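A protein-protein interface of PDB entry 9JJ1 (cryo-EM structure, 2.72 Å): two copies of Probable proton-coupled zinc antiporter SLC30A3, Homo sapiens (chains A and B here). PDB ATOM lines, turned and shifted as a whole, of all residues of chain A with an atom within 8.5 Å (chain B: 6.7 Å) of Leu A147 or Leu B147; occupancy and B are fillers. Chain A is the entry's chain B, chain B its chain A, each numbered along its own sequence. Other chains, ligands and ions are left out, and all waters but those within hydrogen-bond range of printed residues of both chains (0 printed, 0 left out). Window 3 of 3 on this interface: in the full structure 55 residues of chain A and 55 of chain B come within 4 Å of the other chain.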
ATOM      1  N   ARG A 140     -16.449 -20.846  12.190  1.00  0.00           N
ATOM      2  CA  ARG A 140     -16.333 -19.578  12.899  1.00  0.00           C
ATOM      3  C   ARG A 140     -17.673 -18.872  13.055  1.00  0.00           C
ATOM      4  O   ARG A 140     -17.764 -17.902  13.820  1.00  0.00           O
ATOM      5  CB  ARG A 140     -15.341 -18.676  12.166  1.00  0.00           C
ATOM      6  CG  ARG A 140     -14.665 -17.639  13.036  1.00  0.00           C
ATOM      7  CD  ARG A 140     -13.999 -18.259  14.242  1.00  0.00           C
ATOM      8  NE  ARG A 140     -12.643 -18.713  13.962  1.00  0.00           N
ATOM      9  CZ  ARG A 140     -11.562 -17.955  14.080  1.00  0.00           C
ATOM     10  NH1 ARG A 140     -11.644 -16.685  14.431  1.00  0.00           N
ATOM     11  NH2 ARG A 140     -10.369 -18.486  13.839  1.00  0.00           N
ATOM     12  N   SER A 141     -18.708 -19.335  12.351  1.00  0.00           N
ATOM     13  CA  SER A 141     -20.026 -18.727  12.474  1.00  0.00           C
ATOM     14  C   SER A 141     -20.579 -18.872  13.882  1.00  0.00           C
ATOM     15  O   SER A 141     -21.296 -17.990  14.356  1.00  0.00           O
ATOM     16  CB  SER A 141     -20.985 -19.349  11.463  1.00  0.00           C
ATOM     17  OG  SER A 141     -21.097 -20.745  11.666  1.00  0.00           O
ATOM     18  N   GLU A 142     -20.262 -19.973  14.564  1.00  0.00           N
ATOM     19  CA  GLU A 142     -20.726 -20.155  15.935  1.00  0.00           C
ATOM     20  C   GLU A 142     -20.140 -19.094  16.860  1.00  0.00           C
ATOM     21  O   GLU A 142     -20.857 -18.478  17.660  1.00  0.00           O
ATOM     22  CB  GLU A 142     -20.366 -21.560  16.413  1.00  0.00           C
ATOM     23  CG  GLU A 142     -20.175 -21.692  17.906  1.00  0.00           C
ATOM     24  CD  GLU A 142     -19.763 -23.092  18.308  1.00  0.00           C
ATOM     25  OE1 GLU A 142     -19.989 -24.028  17.513  1.00  0.00           O
ATOM     26  OE2 GLU A 142     -19.213 -23.259  19.416  1.00  0.00           O
ATOM     27  N   THR A 143     -18.831 -18.857  16.752  1.00  0.00           N
ATOM     28  CA  THR A 143     -18.194 -17.823  17.559  1.00  0.00           C
ATOM     29  C   THR A 143     -18.736 -16.444  17.214  1.00  0.00           C
ATOM     30  O   THR A 143     -18.971 -15.617  18.105  1.00  0.00           O
ATOM     31  CB  THR A 143     -16.682 -17.866  17.361  1.00  0.00           C
ATOM     32  OG1 THR A 143     -16.241 -19.227  17.352  1.00  0.00           O
ATOM     33  CG2 THR A 143     -15.979 -17.123  18.478  1.00  0.00           C
ATOM     34  N   LEU A 144     -18.938 -16.175  15.924  1.00  0.00           N
ATOM     35  CA  LEU A 144     -19.469 -14.874  15.528  1.00  0.00           C
ATOM     36  C   LEU A 144     -20.884 -14.671  16.057  1.00  0.00           C
ATOM     37  O   LEU A 144     -21.240 -13.568  16.486  1.00  0.00           O
ATOM     38  CB  LEU A 144     -19.426 -14.733  14.009  1.00  0.00           C
ATOM     39  CG  LEU A 144     -18.043 -14.455  13.415  1.00  0.00           C
ATOM     40  CD1 LEU A 144     -18.168 -13.663  12.133  1.00  0.00           C
ATOM     41  CD2 LEU A 144     -17.161 -13.719  14.404  1.00  0.00           C
ATOM     42  N   GLY A 145     -21.701 -15.724  16.045  1.00  0.00           N
ATOM     43  CA  GLY A 145     -23.040 -15.617  16.599  1.00  0.00           C
ATOM     44  C   GLY A 145     -23.035 -15.397  18.099  1.00  0.00           C
ATOM     45  O   GLY A 145     -23.846 -14.630  18.624  1.00  0.00           O
ATOM     46  N   ALA A 146     -22.126 -16.068  18.810  1.00  0.00           N
ATOM     47  CA  ALA A 146     -22.001 -15.825  20.244  1.00  0.00           C
ATOM     48  C   ALA A 146     -21.610 -14.380  20.523  1.00  0.00           C
ATOM     49  O   ALA A 146     -22.169 -13.733  21.420  1.00  0.00           O
ATOM     50  CB  ALA A 146     -20.981 -16.784  20.853  1.00  0.00           C
ATOM     51  N   LEU A 147     -20.658 -13.851  19.751  1.00  0.00           N
ATOM     52  CA  LEU A 147     -20.263 -12.456  19.918  1.00  0.00           C
ATOM     53  C   LEU A 147     -21.424 -11.516  19.624  1.00  0.00           C
ATOM     54  O   LEU A 147     -21.620 -10.519  20.328  1.00  0.00           O
ATOM     55  CB  LEU A 147     -19.075 -12.137  19.016  1.00  0.00           C
ATOM     56  CG  LEU A 147     -18.569 -10.697  19.069  1.00  0.00           C
ATOM     57  CD1 LEU A 147     -17.857 -10.435  20.380  1.00  0.00           C
ATOM     58  CD2 LEU A 147     -17.654 -10.411  17.895  1.00  0.00           C
ATOM     59  N   ALA A 148     -22.200 -11.814  18.579  1.00  0.00           N
ATOM     60  CA  ALA A 148     -23.347 -10.977  18.245  1.00  0.00           C
ATOM     61  C   ALA A 148     -24.379 -10.984  19.364  1.00  0.00           C
ATOM     62  O   ALA A 148     -24.950  -9.940  19.699  1.00  0.00           O
ATOM     63  CB  ALA A 148     -23.973 -11.448  16.934  1.00  0.00           C
ATOM     64  N   SER A 149     -24.637 -12.156  19.947  1.00  0.00           N
ATOM     65  CA  SER A 149     -25.582 -12.231  21.056  1.00  0.00           C
ATOM     66  C   SER A 149     -25.091 -11.424  22.250  1.00  0.00           C
ATOM     67  O   SER A 149     -25.873 -10.708  22.890  1.00  0.00           O
ATOM     68  CB  SER A 149     -25.815 -13.687  21.449  1.00  0.00           C
ATOM     69  OG  SER A 149     -24.749 -14.171  22.244  1.00  0.00           O
ATOM     70  N   VAL A 150     -23.796 -11.517  22.560  1.00  0.00           N
ATOM     71  CA  VAL A 150     -23.248 -10.745  23.673  1.00  0.00           C
ATOM     72  C   VAL A 150     -23.390  -9.251  23.410  1.00  0.00           C
ATOM     73  O   VAL A 150     -23.773  -8.480  24.302  1.00  0.00           O
ATOM     74  CB  VAL A 150     -21.780 -11.141  23.923  1.00  0.00           C
ATOM     75  CG1 VAL A 150     -21.039 -10.027  24.639  1.00  0.00           C
ATOM     76  CG2 VAL A 150     -21.711 -12.428  24.721  1.00  0.00           C
ATOM     77  N   VAL A 151     -23.094  -8.818  22.185  1.00  0.00           N
ATOM     78  CA  VAL A 151     -23.179  -7.399  21.853  1.00  0.00           C
ATOM     79  C   VAL A 151     -24.617  -6.907  21.953  1.00  0.00           C
ATOM     80  O   VAL A 151     -24.881  -5.814  22.469  1.00  0.00           O
ATOM     81  CB  VAL A 151     -22.585  -7.143  20.455  1.00  0.00           C
ATOM     82  CG1 VAL A 151     -23.000  -5.780  19.938  1.00  0.00           C
ATOM     83  CG2 VAL A 151     -21.075  -7.256  20.503  1.00  0.00           C
ATOM     84  N   SER A 152     -25.571  -7.698  21.455  1.00  0.00           N
ATOM     85  CA  SER A 152     -26.974  -7.303  21.544  1.00  0.00           C
ATOM     86  C   SER A 152     -27.430  -7.211  22.994  1.00  0.00           C
ATOM     87  O   SER A 152     -28.177  -6.293  23.365  1.00  0.00           O
ATOM     88  CB  SER A 152     -27.844  -8.291  20.770  1.00  0.00           C
ATOM     89  OG  SER A 152     -28.143  -9.424  21.563  1.00  0.00           O
ATOM     90  N   LEU A 153     -26.999  -8.160  23.827  1.00  0.00           N
ATOM     91  CA  LEU A 153     -27.329  -8.092  25.244  1.00  0.00           C
ATOM     92  C   LEU A 153     -26.769  -6.827  25.873  1.00  0.00           C
ATOM     93  O   LEU A 153     -27.450  -6.165  26.663  1.00  0.00           O
ATOM     94  CB  LEU A 153     -26.800  -9.329  25.967  1.00  0.00           C
ATOM     95  CG  LEU A 153     -26.838  -9.269  27.494  1.00  0.00           C
ATOM     96  CD1 LEU A 153     -28.270  -9.241  27.989  1.00  0.00           C
ATOM     97  CD2 LEU A 153     -26.089 -10.442  28.088  1.00  0.00           C
ATOM     98  N   TRP A 154     -25.527  -6.473  25.530  1.00  0.00           N
ATOM     99  CA  TRP A 154     -24.944  -5.240  26.053  1.00  0.00           C
ATOM    100  C   TRP A 154     -25.740  -4.022  25.604  1.00  0.00           C
ATOM    101  O   TRP A 154     -25.968  -3.099  26.392  1.00  0.00           O
ATOM    102  CB  TRP A 154     -23.488  -5.113  25.610  1.00  0.00           C
ATOM    103  CG  TRP A 154     -22.516  -5.754  26.545  1.00  0.00           C
ATOM    104  CD1 TRP A 154     -22.256  -7.083  26.665  1.00  0.00           C
ATOM    105  CD2 TRP A 154     -21.673  -5.093  27.494  1.00  0.00           C
ATOM    106  NE1 TRP A 154     -21.300  -7.295  27.626  1.00  0.00           N
ATOM    107  CE2 TRP A 154     -20.927  -6.088  28.153  1.00  0.00           C
ATOM    108  CE3 TRP A 154     -21.476  -3.755  27.852  1.00  0.00           C
ATOM    109  CZ2 TRP A 154     -20.000  -5.790  29.149  1.00  0.00           C
ATOM    110  CZ3 TRP A 154     -20.556  -3.461  28.842  1.00  0.00           C
ATOM    111  CH2 TRP A 154     -19.829  -4.473  29.478  1.00  0.00           C
ATOM    112  N   THR A 281     -22.328 -12.329  31.437  1.00  0.00           N
ATOM    113  CA  THR A 281     -21.891 -12.346  30.048  1.00  0.00           C
ATOM    114  C   THR A 281     -20.396 -12.101  29.884  1.00  0.00           C
ATOM    115  O   THR A 281     -19.867 -12.347  28.795  1.00  0.00           O
ATOM    116  CB  THR A 281     -22.667 -11.307  29.234  1.00  0.00           C
ATOM    117  OG1 THR A 281     -22.721 -11.719  27.864  1.00  0.00           O
ATOM    118  CG2 THR A 281     -21.997  -9.952  29.311  1.00  0.00           C
ATOM    119  N   THR A 284     -18.161 -15.385  28.717  1.00  0.00           N
ATOM    120  CA  THR A 284     -18.355 -15.771  27.324  1.00  0.00           C
ATOM    121  C   THR A 284     -17.668 -14.789  26.391  1.00  0.00           C
ATOM    122  O   THR A 284     -17.084 -15.188  25.378  1.00  0.00           O
ATOM    123  CB  THR A 284     -19.843 -15.862  27.000  1.00  0.00           C
ATOM    124  OG1 THR A 284     -20.414 -14.548  27.003  1.00  0.00           O
ATOM    125  CG2 THR A 284     -20.558 -16.720  28.028  1.00  0.00           C
ATOM    126  N   LEU A 285     -17.726 -13.497  26.719  1.00  0.00           N
ATOM    127  CA  LEU A 285     -17.021 -12.502  25.921  1.00  0.00           C
ATOM    128  C   LEU A 285     -15.519 -12.741  25.959  1.00  0.00           C
ATOM    129  O   LEU A 285     -14.840 -12.624  24.934  1.00  0.00           O
ATOM    130  CB  LEU A 285     -17.356 -11.099  26.421  1.00  0.00           C
ATOM    131  CG  LEU A 285     -16.486  -9.953  25.901  1.00  0.00           C
ATOM    132  CD1 LEU A 285     -16.556  -9.871  24.387  1.00  0.00           C
ATOM    133  CD2 LEU A 285     -16.907  -8.638  26.528  1.00  0.00           C
ATOM    134  N   ARG A 286     -14.984 -13.082  27.132  1.00  0.00           N
ATOM    135  CA  ARG A 286     -13.556 -13.368  27.236  1.00  0.00           C
ATOM    136  C   ARG A 286     -13.168 -14.556  26.364  1.00  0.00           C
ATOM    137  O   ARG A 286     -12.167 -14.510  25.636  1.00  0.00           O
ATOM    138  CB  ARG A 286     -13.183 -13.626  28.694  1.00  0.00           C
ATOM    139  CG  ARG A 286     -11.728 -13.355  29.019  1.00  0.00           C
ATOM    140  CD  ARG A 286     -11.156 -14.435  29.918  1.00  0.00           C
ATOM    141  NE  ARG A 286     -12.155 -14.971  30.835  1.00  0.00           N
ATOM    142  CZ  ARG A 286     -12.470 -16.255  30.930  1.00  0.00           C
ATOM    143  NH1 ARG A 286     -11.886 -17.169  30.172  1.00  0.00           N
ATOM    144  NH2 ARG A 286     -13.396 -16.632  31.808  1.00  0.00           N
ATOM    145  N   ASP A 287     -13.957 -15.630  26.420  1.00  0.00           N
ATOM    146  CA  ASP A 287     -13.653 -16.812  25.617  1.00  0.00           C
ATOM    147  C   ASP A 287     -13.746 -16.513  24.126  1.00  0.00           C
ATOM    148  O   ASP A 287     -12.891 -16.942  23.340  1.00  0.00           O
ATOM    149  CB  ASP A 287     -14.597 -17.952  25.993  1.00  0.00           C
ATOM    150  CG  ASP A 287     -14.048 -18.814  27.109  1.00  0.00           C
ATOM    151  OD1 ASP A 287     -12.916 -18.548  27.563  1.00  0.00           O
ATOM    152  OD2 ASP A 287     -14.750 -19.755  27.535  1.00  0.00           O
ATOM    153  N   VAL A 288     -14.781 -15.775  23.718  1.00  0.00           N
ATOM    154  CA  VAL A 288     -14.950 -15.435  22.310  1.00  0.00           C
ATOM    155  C   VAL A 288     -13.791 -14.576  21.827  1.00  0.00           C
ATOM    156  O   VAL A 288     -13.270 -14.776  20.724  1.00  0.00           O
ATOM    157  CB  VAL A 288     -16.306 -14.738  22.094  1.00  0.00           C
ATOM    158  CG1 VAL A 288     -16.290 -13.914  20.822  1.00  0.00           C
ATOM    159  CG2 VAL A 288     -17.421 -15.763  22.051  1.00  0.00           C
ATOM    160  N   LEU A 289     -13.371 -13.602  22.638  1.00  0.00           N
ATOM    161  CA  LEU A 289     -12.244 -12.760  22.258  1.00  0.00           C
ATOM    162  C   LEU A 289     -10.965 -13.573  22.137  1.00  0.00           C
ATOM    163  O   LEU A 289     -10.168 -13.355  21.219  1.00  0.00           O
ATOM    164  CB  LEU A 289     -12.064 -11.633  23.271  1.00  0.00           C
ATOM    165  CG  LEU A 289     -12.999 -10.436  23.121  1.00  0.00           C
ATOM    166  CD1 LEU A 289     -12.416  -9.227  23.825  1.00  0.00           C
ATOM    167  CD2 LEU A 289     -13.258 -10.135  21.657  1.00  0.00           C
ATOM    168  N   LEU A 292     -11.173 -15.425  18.861  1.00  0.00           N
ATOM    169  CA  LEU A 292     -11.101 -14.567  17.684  1.00  0.00           C
ATOM    170  C   LEU A 292      -9.716 -13.970  17.493  1.00  0.00           C
ATOM    171  O   LEU A 292      -9.293 -13.753  16.354  1.00  0.00           O
ATOM    172  CB  LEU A 292     -12.142 -13.455  17.781  1.00  0.00           C
ATOM    173  CG  LEU A 292     -13.577 -13.832  17.420  1.00  0.00           C
ATOM    174  CD1 LEU A 292     -14.445 -12.594  17.364  1.00  0.00           C
ATOM    175  CD2 LEU A 292     -13.622 -14.577  16.103  1.00  0.00           C
ATOM    176  N   GLU B 142      -6.125  -5.231  15.433  1.00  0.00           N
ATOM    177  CA  GLU B 142      -6.555  -4.208  14.486  1.00  0.00           C
ATOM    178  C   GLU B 142      -7.933  -4.530  13.919  1.00  0.00           C
ATOM    179  O   GLU B 142      -8.813  -3.661  13.847  1.00  0.00           O
ATOM    180  CB  GLU B 142      -5.517  -4.073  13.374  1.00  0.00           C
ATOM    181  CG  GLU B 142      -6.084  -3.744  12.011  1.00  0.00           C
ATOM    182  CD  GLU B 142      -5.005  -3.632  10.956  1.00  0.00           C
ATOM    183  OE1 GLU B 142      -3.812  -3.695  11.317  1.00  0.00           O
ATOM    184  OE2 GLU B 142      -5.348  -3.485   9.764  1.00  0.00           O
ATOM    185  N   THR B 143      -8.145  -5.787  13.525  1.00  0.00           N
ATOM    186  CA  THR B 143      -9.453  -6.197  13.026  1.00  0.00           C
ATOM    187  C   THR B 143     -10.515  -6.085  14.109  1.00  0.00           C
ATOM    188  O   THR B 143     -11.640  -5.642  13.846  1.00  0.00           O
ATOM    189  CB  THR B 143      -9.382  -7.627  12.493  1.00  0.00           C
ATOM    190  OG1 THR B 143      -8.180  -7.793  11.734  1.00  0.00           O
ATOM    191  CG2 THR B 143     -10.575  -7.922  11.609  1.00  0.00           C
ATOM    192  N   LEU B 144     -10.176  -6.483  15.336  1.00  0.00           N
ATOM    193  CA  LEU B 144     -11.144  -6.388  16.423  1.00  0.00           C
ATOM    194  C   LEU B 144     -11.502  -4.936  16.715  1.00  0.00           C
ATOM    195  O   LEU B 144     -12.665  -4.620  16.992  1.00  0.00           O
ATOM    196  CB  LEU B 144     -10.600  -7.079  17.670  1.00  0.00           C
ATOM    197  CG  LEU B 144     -10.636  -8.609  17.640  1.00  0.00           C
ATOM    198  CD1 LEU B 144     -10.773  -9.160  19.041  1.00  0.00           C
ATOM    199  CD2 LEU B 144     -11.765  -9.113  16.763  1.00  0.00           C
ATOM    200  N   GLY B 145     -10.522  -4.035  16.652  1.00  0.00           N
ATOM    201  CA  GLY B 145     -10.809  -2.626  16.851  1.00  0.00           C
ATOM    202  C   GLY B 145     -11.673  -2.045  15.750  1.00  0.00           C
ATOM    203  O   GLY B 145     -12.561  -1.227  16.012  1.00  0.00           O
ATOM    204  N   ALA B 146     -11.426  -2.451  14.503  1.00  0.00           N
ATOM    205  CA  ALA B 146     -12.287  -2.008  13.409  1.00  0.00           C
ATOM    206  C   ALA B 146     -13.720  -2.484  13.614  1.00  0.00           C
ATOM    207  O   ALA B 146     -14.676  -1.720  13.418  1.00  0.00           O
ATOM    208  CB  ALA B 146     -11.740  -2.509  12.075  1.00  0.00           C
ATOM    209  N   LEU B 147     -13.887  -3.743  14.023  1.00  0.00           N
ATOM    210  CA  LEU B 147     -15.224  -4.258  14.293  1.00  0.00           C
ATOM    211  C   LEU B 147     -15.889  -3.498  15.432  1.00  0.00           C
ATOM    212  O   LEU B 147     -17.087  -3.196  15.372  1.00  0.00           O
ATOM    213  CB  LEU B 147     -15.156  -5.749  14.615  1.00  0.00           C
ATOM    214  CG  LEU B 147     -16.488  -6.419  14.944  1.00  0.00           C
ATOM    215  CD1 LEU B 147     -17.335  -6.556  13.696  1.00  0.00           C
ATOM    216  CD2 LEU B 147     -16.259  -7.770  15.588  1.00  0.00           C
ATOM    217  N   ALA B 148     -15.127  -3.187  16.483  1.00  0.00           N
ATOM    218  CA  ALA B 148     -15.681  -2.437  17.605  1.00  0.00           C
ATOM    219  C   ALA B 148     -16.130  -1.049  17.174  1.00  0.00           C
ATOM    220  O   ALA B 148     -17.190  -0.571  17.593  1.00  0.00           O
ATOM    221  CB  ALA B 148     -14.653  -2.343  18.730  1.00  0.00           C
ATOM    222  N   SER B 149     -15.331  -0.383  16.338  1.00  0.00           N
ATOM    223  CA  SER B 149     -15.718   0.935  15.848  1.00  0.00           C
ATOM    224  C   SER B 149     -16.991   0.859  15.016  1.00  0.00           C
ATOM    225  O   SER B 149     -17.884   1.705  15.152  1.00  0.00           O
ATOM    226  CB  SER B 149     -14.581   1.549  15.034  1.00  0.00           C
ATOM    227  OG  SER B 149     -14.543   1.003  13.729  1.00  0.00           O
ATOM    228  N   VAL B 150     -17.098  -0.157  14.156  1.00  0.00           N
ATOM    229  CA  VAL B 150     -18.306  -0.315  13.347  1.00  0.00           C
ATOM    230  C   VAL B 150     -19.521  -0.542  14.239  1.00  0.00           C
ATOM    231  O   VAL B 150     -20.591   0.042  14.022  1.00  0.00           O
ATOM    232  CB  VAL B 150     -18.121  -1.458  12.333  1.00  0.00           C
ATOM    233  CG1 VAL B 150     -19.467  -2.009  11.897  1.00  0.00           C
ATOM    234  CG2 VAL B 150     -17.329  -0.976  11.134  1.00  0.00           C
ATOM    235  N   VAL B 151     -19.375  -1.388  15.260  1.00  0.00           N
ATOM    236  CA  VAL B 151     -20.494  -1.684  16.151  1.00  0.00           C
ATOM    237  C   VAL B 151     -20.920  -0.437  16.915  1.00  0.00           C
ATOM    238  O   VAL B 151     -22.117  -0.168  17.076  1.00  0.00           O
ATOM    239  CB  VAL B 151     -20.124  -2.837  17.102  1.00  0.00           C
ATOM    240  CG1 VAL B 151     -21.097  -2.906  18.264  1.00  0.00           C
ATOM    241  CG2 VAL B 151     -20.107  -4.150  16.347  1.00  0.00           C
ATOM    242  N   SER B 152     -19.952   0.341  17.406  1.00  0.00           N
ATOM    243  CA  SER B 152     -20.287   1.567  18.123  1.00  0.00           C
ATOM    244  C   SER B 152     -20.996   2.562  17.213  1.00  0.00           C
ATOM    245  O   SER B 152     -21.952   3.233  17.631  1.00  0.00           O
ATOM    246  CB  SER B 152     -19.025   2.189  18.714  1.00  0.00           C
ATOM    247  OG  SER B 152     -18.349   2.971  17.747  1.00  0.00           O
ATOM    248  N   LEU B 285     -17.419  -3.539   7.337  1.00  0.00           N
ATOM    249  CA  LEU B 285     -17.983  -4.668   8.066  1.00  0.00           C
ATOM    250  C   LEU B 285     -17.847  -5.955   7.268  1.00  0.00           C
ATOM    251  O   LEU B 285     -17.525  -7.009   7.827  1.00  0.00           O
ATOM    252  CB  LEU B 285     -19.448  -4.397   8.401  1.00  0.00           C
ATOM    253  CG  LEU B 285     -20.249  -5.584   8.933  1.00  0.00           C
ATOM    254  CD1 LEU B 285     -19.652  -6.090  10.234  1.00  0.00           C
ATOM    255  CD2 LEU B 285     -21.704  -5.205   9.123  1.00  0.00           C
ATOM    256  N   VAL B 288     -14.168  -7.042   7.461  1.00  0.00           N
ATOM    257  CA  VAL B 288     -13.841  -7.531   8.795  1.00  0.00           C
ATOM    258  C   VAL B 288     -14.440  -8.911   9.020  1.00  0.00           C
ATOM    259  O   VAL B 288     -13.791  -9.800   9.581  1.00  0.00           O
ATOM    260  CB  VAL B 288     -14.313  -6.523   9.859  1.00  0.00           C
ATOM    261  CG1 VAL B 288     -14.484  -7.199  11.203  1.00  0.00           C
ATOM    262  CG2 VAL B 288     -13.332  -5.374   9.964  1.00  0.00           C
ATOM    263  N   LEU B 289     -15.689  -9.112   8.594  1.00  0.00           N
ATOM    264  CA  LEU B 289     -16.318 -10.418   8.745  1.00  0.00           C
ATOM    265  C   LEU B 289     -15.587 -11.477   7.935  1.00  0.00           C
ATOM    266  O   LEU B 289     -15.407 -12.608   8.400  1.00  0.00           O
ATOM    267  CB  LEU B 289     -17.785 -10.345   8.328  1.00  0.00           C
ATOM    268  CG  LEU B 289     -18.751  -9.764   9.357  1.00  0.00           C
ATOM    269  CD1 LEU B 289     -20.169 -10.194   9.040  1.00  0.00           C
ATOM    270  CD2 LEU B 289     -18.360 -10.188  10.762  1.00  0.00           C
ATOM    271  N   LEU B 292     -12.468 -12.344   9.861  1.00  0.00           N
ATOM    272  CA  LEU B 292     -12.714 -13.041  11.119  1.00  0.00           C
ATOM    273  C   LEU B 292     -13.220 -14.458  10.899  1.00  0.00           C
ATOM    274  O   LEU B 292     -12.927 -15.345  11.706  1.00  0.00           O
ATOM    275  CB  LEU B 292     -13.709 -12.256  11.967  1.00  0.00           C
ATOM    276  CG  LEU B 292     -13.156 -11.053  12.728  1.00  0.00           C
ATOM    277  CD1 LEU B 292     -14.204 -10.502  13.672  1.00  0.00           C
ATOM    278  CD2 LEU B 292     -11.899 -11.428  13.483  1.00  0.00           C
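Leu A144 touches Leu B289 (CD1 to CD2, 3.7 Å).
CD2 of Leu B147 touches CD2 of Leu A147 (3.8 Å).
Val A151 touches Val B151 (CG1 to CG1, 3.8 Å).
Leu A289 touches Leu B144.
Leu A144 touches Leu B289, and with the chains exchanged Leu A289 touches Leu B144.
Leu A147 touches its own counterpart, Leu B147.
Val A151 touches its own counterpart, Val B151.
15 positions are printed for both chains.
Of the 5 pairs that touch across the chains among the printed residues, 4 have their exchanged pair printed and touching as well.
Of the 15 printed residues of chain B, 5 touch a printed residue of chain A.
Of the 23 printed residues of chain A, 5 touch a printed residue of chain B.
Hydrophobic or aromatic side chains of chain A within 4 Å of the printed part of chain B: Leu A144, Leu A147, Val A151 and Leu A289.
NH1 of Arg A140 sits close to O of Leu B292 (3.3 Å).
Of chain B, only Leu B147 comes within 4 Å of Leu A147.
Of chain A, only Leu A147 (3.8 Å) comes within 4 Å of Leu B147.
No residue of chain A comes within 4 Å of Gly B145.
No residue of chain A comes within 4 Å of Ala B146.
Of the printed residues of chain A, Leu B289 touches Leu A144.
Of the printed residues of chain B, Leu A289 touches Leu B144.
Of the printed residues of chain A, Leu B292 touches Arg A140.
Leu A153 touches none of the printed residues of chain B.
Ser A149 touches none of the printed residues of chain B.
The nearest residue of chain B that does not touch Leu A147 is Leu B292 (5.5 Å).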
